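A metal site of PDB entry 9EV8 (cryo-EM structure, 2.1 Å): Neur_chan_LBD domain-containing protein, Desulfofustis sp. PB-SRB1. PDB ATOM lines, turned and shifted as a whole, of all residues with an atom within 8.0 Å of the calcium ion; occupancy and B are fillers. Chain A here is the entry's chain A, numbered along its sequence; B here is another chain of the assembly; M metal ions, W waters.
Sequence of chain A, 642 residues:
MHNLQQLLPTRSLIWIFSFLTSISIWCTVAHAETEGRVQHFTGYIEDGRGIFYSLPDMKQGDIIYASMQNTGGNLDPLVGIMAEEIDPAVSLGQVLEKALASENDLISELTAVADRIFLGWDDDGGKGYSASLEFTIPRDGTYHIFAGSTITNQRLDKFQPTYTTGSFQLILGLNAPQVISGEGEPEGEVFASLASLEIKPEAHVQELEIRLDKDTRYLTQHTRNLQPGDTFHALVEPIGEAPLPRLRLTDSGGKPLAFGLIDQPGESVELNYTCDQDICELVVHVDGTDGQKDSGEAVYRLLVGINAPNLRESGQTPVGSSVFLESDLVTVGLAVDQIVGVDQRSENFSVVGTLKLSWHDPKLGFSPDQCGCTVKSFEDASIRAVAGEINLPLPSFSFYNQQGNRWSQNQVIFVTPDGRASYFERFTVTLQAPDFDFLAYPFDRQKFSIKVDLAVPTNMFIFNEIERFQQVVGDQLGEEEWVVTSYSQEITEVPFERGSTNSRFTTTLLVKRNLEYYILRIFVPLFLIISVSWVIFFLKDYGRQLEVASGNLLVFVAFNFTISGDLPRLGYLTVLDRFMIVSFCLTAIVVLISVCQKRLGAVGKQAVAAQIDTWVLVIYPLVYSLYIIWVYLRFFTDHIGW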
ATOM      1  N   GLN A 344      16.588 -12.520  10.421  1.00  0.00           N
ATOM      2  CA  GLN A 344      16.610 -11.766  11.671  1.00  0.00           C
ATOM      3  C   GLN A 344      15.245 -11.200  12.058  1.00  0.00           C
ATOM      4  O   GLN A 344      15.082 -10.778  13.210  1.00  0.00           O
ATOM      5  CB  GLN A 344      17.622 -10.622  11.570  1.00  0.00           C
ATOM      6  CG  GLN A 344      19.047 -11.100  11.354  1.00  0.00           C
ATOM      7  CD  GLN A 344      20.039  -9.959  11.228  1.00  0.00           C
ATOM      8  OE1 GLN A 344      21.247 -10.174  11.187  1.00  0.00           O
ATOM      9  NE2 GLN A 344      19.530  -8.735  11.151  1.00  0.00           N
ATOM     10  N   ARG A 345      14.282 -11.177  11.148  1.00  0.00           N
ATOM     11  CA  ARG A 345      12.947 -10.707  11.499  1.00  0.00           C
ATOM     12  C   ARG A 345      12.046 -11.832  11.990  1.00  0.00           C
ATOM     13  O   ARG A 345      11.307 -11.651  12.972  1.00  0.00           O
ATOM     14  CB  ARG A 345      12.291 -10.011  10.310  1.00  0.00           C
ATOM     15  CG  ARG A 345      12.771  -8.590  10.089  1.00  0.00           C
ATOM     16  CD  ARG A 345      11.968  -7.893   9.000  1.00  0.00           C
ATOM     17  NE  ARG A 345      10.543  -7.881   9.299  1.00  0.00           N
ATOM     18  CZ  ARG A 345       9.929  -6.955  10.023  1.00  0.00           C
ATOM     19  NH1 ARG A 345      10.585  -5.941  10.542  1.00  0.00           N
ATOM     20  NH2 ARG A 345       8.611  -7.046  10.220  1.00  0.00           N
ATOM     21  N   SER A 346      12.077 -12.994  11.339  1.00  0.00           N
ATOM     22  CA  SER A 346      11.296 -14.142  11.756  1.00  0.00           C
ATOM     23  C   SER A 346      12.044 -15.049  12.721  1.00  0.00           C
ATOM     24  O   SER A 346      11.440 -15.991  13.253  1.00  0.00           O
ATOM     25  CB  SER A 346      10.857 -14.948  10.520  1.00  0.00           C
ATOM     26  OG  SER A 346      10.090 -16.078  10.896  1.00  0.00           O
ATOM     27  N   GLU A 347      13.327 -14.777  12.972  1.00  0.00           N
ATOM     28  CA  GLU A 347      14.137 -15.505  13.949  1.00  0.00           C
ATOM     29  C   GLU A 347      14.193 -17.000  13.640  1.00  0.00           C
ATOM     30  O   GLU A 347      13.714 -17.849  14.390  1.00  0.00           O
ATOM     31  CB  GLU A 347      13.625 -15.246  15.372  1.00  0.00           C
ATOM     32  CG  GLU A 347      13.611 -13.770  15.745  1.00  0.00           C
ATOM     33  CD  GLU A 347      13.403 -13.535  17.231  1.00  0.00           C
ATOM     34  OE1 GLU A 347      13.566 -14.497  18.013  1.00  0.00           O
ATOM     35  OE2 GLU A 347      13.084 -12.391  17.623  1.00  0.00           O
ATOM     36  N   ALA A 433      14.290 -20.212  15.904  1.00  0.00           N
ATOM     37  CA  ALA A 433      15.188 -19.828  16.980  1.00  0.00           C
ATOM     38  C   ALA A 433      14.679 -18.578  17.704  1.00  0.00           C
ATOM     39  O   ALA A 433      15.240 -17.492  17.540  1.00  0.00           O
ATOM     40  CB  ALA A 433      16.589 -19.575  16.440  1.00  0.00           C
ATOM     41  N   PRO A 434      13.624 -18.697  18.523  1.00  0.00           N
ATOM     42  CA  PRO A 434      13.113 -17.521  19.227  1.00  0.00           C
ATOM     43  C   PRO A 434      14.054 -16.971  20.297  1.00  0.00           C
ATOM     44  O   PRO A 434      13.790 -15.897  20.843  1.00  0.00           O
ATOM     45  CB  PRO A 434      11.804 -18.028  19.852  1.00  0.00           C
ATOM     46  CG  PRO A 434      11.988 -19.491  19.964  1.00  0.00           C
ATOM     47  CD  PRO A 434      12.808 -19.901  18.785  1.00  0.00           C
ATOM     48  N   ASP A 435      15.139 -17.688  20.623  1.00  0.00           N
ATOM     49  CA  ASP A 435      16.073 -17.219  21.637  1.00  0.00           C
ATOM     50  C   ASP A 435      16.975 -16.084  21.160  1.00  0.00           C
ATOM     51  O   ASP A 435      17.737 -15.551  21.974  1.00  0.00           O
ATOM     52  CB  ASP A 435      16.928 -18.378  22.146  1.00  0.00           C
ATOM     53  CG  ASP A 435      16.115 -19.397  22.920  1.00  0.00           C
ATOM     54  OD1 ASP A 435      14.881 -19.207  23.058  1.00  0.00           O
ATOM     55  OD2 ASP A 435      16.700 -20.396  23.396  1.00  0.00           O
ATOM     56  N   PHE A 436      16.927 -15.720  19.875  1.00  0.00           N
ATOM     57  CA  PHE A 436      17.767 -14.645  19.348  1.00  0.00           C
ATOM     58  C   PHE A 436      17.510 -13.334  20.095  1.00  0.00           C
ATOM     59  O   PHE A 436      16.376 -13.030  20.461  1.00  0.00           O
ATOM     60  CB  PHE A 436      17.509 -14.450  17.856  1.00  0.00           C
ATOM     61  CG  PHE A 436      18.134 -15.492  16.980  1.00  0.00           C
ATOM     62  CD1 PHE A 436      19.143 -16.314  17.461  1.00  0.00           C
ATOM     63  CD2 PHE A 436      17.729 -15.632  15.660  1.00  0.00           C
ATOM     64  CE1 PHE A 436      19.714 -17.273  16.645  1.00  0.00           C
ATOM     65  CE2 PHE A 436      18.303 -16.582  14.845  1.00  0.00           C
ATOM     66  CZ  PHE A 436      19.294 -17.407  15.337  1.00  0.00           C
ATOM     67  N   ASP A 437      18.574 -12.566  20.306  1.00  0.00           N
ATOM     68  CA  ASP A 437      18.491 -11.254  20.937  1.00  0.00           C
ATOM     69  C   ASP A 437      19.466 -10.323  20.227  1.00  0.00           C
ATOM     70  O   ASP A 437      20.683 -10.483  20.357  1.00  0.00           O
ATOM     71  CB  ASP A 437      18.793 -11.338  22.433  1.00  0.00           C
ATOM     72  CG  ASP A 437      18.605 -10.021  23.148  1.00  0.00           C
ATOM     73  OD1 ASP A 437      18.042  -9.080  22.541  1.00  0.00           O
ATOM     74  OD2 ASP A 437      19.012  -9.920  24.319  1.00  0.00           O
ATOM     75  N   PHE A 438      18.941  -9.339  19.495  1.00  0.00           N
ATOM     76  CA  PHE A 438      19.748  -8.424  18.695  1.00  0.00           C
ATOM     77  C   PHE A 438      19.870  -7.043  19.321  1.00  0.00           C
ATOM     78  O   PHE A 438      20.094  -6.074  18.592  1.00  0.00           O
ATOM     79  CB  PHE A 438      19.160  -8.306  17.289  1.00  0.00           C
ATOM     80  CG  PHE A 438      19.076  -9.614  16.560  1.00  0.00           C
ATOM     81  CD1 PHE A 438      20.219 -10.252  16.126  1.00  0.00           C
ATOM     82  CD2 PHE A 438      17.847 -10.197  16.304  1.00  0.00           C
ATOM     83  CE1 PHE A 438      20.146 -11.457  15.445  1.00  0.00           C
ATOM     84  CE2 PHE A 438      17.765 -11.399  15.630  1.00  0.00           C
ATOM     85  CZ  PHE A 438      18.917 -12.031  15.204  1.00  0.00           C
ATOM     86  N   GLN A 446      25.285 -14.884  19.479  1.00  0.00           N
ATOM     87  CA  GLN A 446      24.109 -15.718  19.360  1.00  0.00           C
ATOM     88  C   GLN A 446      24.483 -17.193  19.502  1.00  0.00           C
ATOM     89  O   GLN A 446      25.661 -17.567  19.445  1.00  0.00           O
ATOM     90  CB  GLN A 446      23.388 -15.497  18.024  1.00  0.00           C
ATOM     91  CG  GLN A 446      23.083 -14.043  17.694  1.00  0.00           C
ATOM     92  CD  GLN A 446      22.108 -13.414  18.669  1.00  0.00           C
ATOM     93  OE1 GLN A 446      21.280 -14.099  19.267  1.00  0.00           O
ATOM     94  NE2 GLN A 446      22.197 -12.100  18.827  1.00  0.00           N
ATOM     95  N   TYR A 572      12.487  -2.265  16.955  1.00  0.00           N
ATOM     96  CA  TYR A 572      12.993  -1.810  18.239  1.00  0.00           C
ATOM     97  C   TYR A 572      14.436  -1.338  18.058  1.00  0.00           C
ATOM     98  O   TYR A 572      15.102  -1.684  17.076  1.00  0.00           O
ATOM     99  CB  TYR A 572      12.895  -2.904  19.305  1.00  0.00           C
ATOM    100  CG  TYR A 572      13.447  -4.246  18.884  1.00  0.00           C
ATOM    101  CD1 TYR A 572      14.786  -4.563  19.059  1.00  0.00           C
ATOM    102  CD2 TYR A 572      12.623  -5.203  18.308  1.00  0.00           C
ATOM    103  CE1 TYR A 572      15.288  -5.780  18.684  1.00  0.00           C
ATOM    104  CE2 TYR A 572      13.124  -6.429  17.919  1.00  0.00           C
ATOM    105  CZ  TYR A 572      14.451  -6.710  18.113  1.00  0.00           C
ATOM    106  OH  TYR A 572      14.957  -7.938  17.731  1.00  0.00           O
ATOM    107  N   GLN B 338       5.137 -17.951  19.093  1.00  0.00           N
ATOM    108  CA  GLN B 338       5.826 -16.845  18.440  1.00  0.00           C
ATOM    109  C   GLN B 338       4.974 -16.310  17.297  1.00  0.00           C
ATOM    110  O   GLN B 338       4.417 -17.085  16.522  1.00  0.00           O
ATOM    111  CB  GLN B 338       7.198 -17.291  17.923  1.00  0.00           C
ATOM    112  CG  GLN B 338       7.930 -16.239  17.114  1.00  0.00           C
ATOM    113  CD  GLN B 338       9.190 -16.766  16.473  1.00  0.00           C
ATOM    114  OE1 GLN B 338       9.507 -17.958  16.577  1.00  0.00           O
ATOM    115  NE2 GLN B 338       9.922 -15.891  15.798  1.00  0.00           N
ATOM    116  N   ASP B 475       6.951 -16.407  26.616  1.00  0.00           N
ATOM    117  CA  ASP B 475       8.016 -15.419  26.656  1.00  0.00           C
ATOM    118  C   ASP B 475       9.239 -15.905  25.880  1.00  0.00           C
ATOM    119  O   ASP B 475       9.577 -17.092  25.908  1.00  0.00           O
ATOM    120  CB  ASP B 475       8.413 -15.109  28.106  1.00  0.00           C
ATOM    121  CG  ASP B 475       8.846 -16.348  28.873  1.00  0.00           C
ATOM    122  OD1 ASP B 475       8.347 -17.442  28.560  1.00  0.00           O
ATOM    123  OD2 ASP B 475       9.680 -16.213  29.780  1.00  0.00           O
ATOM    124  N   GLN B 476       9.893 -14.987  25.170  1.00  0.00           N
ATOM    125  CA  GLN B 476      11.061 -15.290  24.373  1.00  0.00           C
ATOM    126  C   GLN B 476      12.150 -14.276  24.652  1.00  0.00           C
ATOM    127  O   GLN B 476      11.858 -13.132  25.026  1.00  0.00           O
ATOM    128  CB  GLN B 476      10.734 -15.292  22.868  1.00  0.00           C
ATOM    129  CG  GLN B 476       9.644 -16.269  22.452  1.00  0.00           C
ATOM    130  CD  GLN B 476      10.076 -17.720  22.537  1.00  0.00           C
ATOM    131  OE1 GLN B 476      11.257 -18.018  22.687  1.00  0.00           O
ATOM    132  NE2 GLN B 476       9.116 -18.629  22.426  1.00  0.00           N
ATOM    133  N   LEU B 477      13.406 -14.689  24.494  1.00  0.00           N
ATOM    134  CA  LEU B 477      14.529 -13.794  24.703  1.00  0.00           C
ATOM    135  C   LEU B 477      14.573 -12.731  23.615  1.00  0.00           C
ATOM    136  O   LEU B 477      14.193 -12.972  22.459  1.00  0.00           O
ATOM    137  CB  LEU B 477      15.848 -14.571  24.730  1.00  0.00           C
ATOM    138  CG  LEU B 477      16.020 -15.611  25.831  1.00  0.00           C
ATOM    139  CD1 LEU B 477      17.338 -16.360  25.656  1.00  0.00           C
ATOM    140  CD2 LEU B 477      15.965 -14.960  27.201  1.00  0.00           C
ATOM    141  N   GLY B 478      15.041 -11.540  23.978  1.00  0.00           N
ATOM    142  CA  GLY B 478      15.123 -10.433  23.037  1.00  0.00           C
ATOM    143  C   GLY B 478      13.823  -9.661  22.934  1.00  0.00           C
ATOM    144  O   GLY B 478      12.815  -9.974  23.565  1.00  0.00           O
ATOM    145  N   GLU B 479      13.870  -8.609  22.125  1.00  0.00           N
ATOM    146  CA  GLU B 479      12.711  -7.769  21.886  1.00  0.00           C
ATOM    147  C   GLU B 479      11.904  -8.282  20.699  1.00  0.00           C
ATOM    148  O   GLU B 479      12.396  -9.026  19.851  1.00  0.00           O
ATOM    149  CB  GLU B 479      13.132  -6.313  21.640  1.00  0.00           C
ATOM    150  CG  GLU B 479      14.021  -5.733  22.730  1.00  0.00           C
ATOM    151  CD  GLU B 479      13.310  -5.606  24.061  1.00  0.00           C
ATOM    152  OE1 GLU B 479      12.062  -5.504  24.071  1.00  0.00           O
ATOM    153  OE2 GLU B 479      13.997  -5.611  25.100  1.00  0.00           O
ATOM    154  N   GLU B 480      10.642  -7.859  20.641  1.00  0.00           N
ATOM    155  CA  GLU B 480       9.742  -8.177  19.549  1.00  0.00           C
ATOM    156  C   GLU B 480       9.135  -6.899  18.997  1.00  0.00           C
ATOM    157  O   GLU B 480       9.048  -5.878  19.693  1.00  0.00           O
ATOM    158  CB  GLU B 480       8.629  -9.142  19.995  1.00  0.00           C
ATOM    159  CG  GLU B 480       9.092 -10.560  20.292  1.00  0.00           C
ATOM    160  CD  GLU B 480       9.688 -10.702  21.685  1.00  0.00           C
ATOM    161  OE1 GLU B 480       9.416  -9.829  22.535  1.00  0.00           O
ATOM    162  OE2 GLU B 480      10.420 -11.686  21.919  1.00  0.00           O
HETATM  163 CA    CA M   1      13.965 -13.432  20.009  1.00  0.00          CA
HETATM  164  O   HOH W   1      14.182 -10.863  19.722  1.00  0.00           O
HETATM  165  O   HOH W   2      12.016 -13.387  20.669  1.00  0.00           O
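The calcium ion is bound by water W2 (2.1 Å), OE1 of Glu 347 (2.3 Å), O of Phe 436 (2.5 Å), O of Leu 477 of chain B (2.5 Å), water W1 (2.6 Å), O of Pro 434 (2.6 Å) and OE2 of Glu 347 (2.7 Å). The calcium ion has seven donor atoms within binding distance.
Four residues have an atom within 4 Å of the calcium ion: Glu 347, Pro 434, Phe 436 and Leu 477 of chain B. The nearest printed residue that does not touch the calcium ion is Asp 435 (4.2 Å).
N of Ala 433 lies within hydrogen-bond range of O of Glu 347 (2.9 Å).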
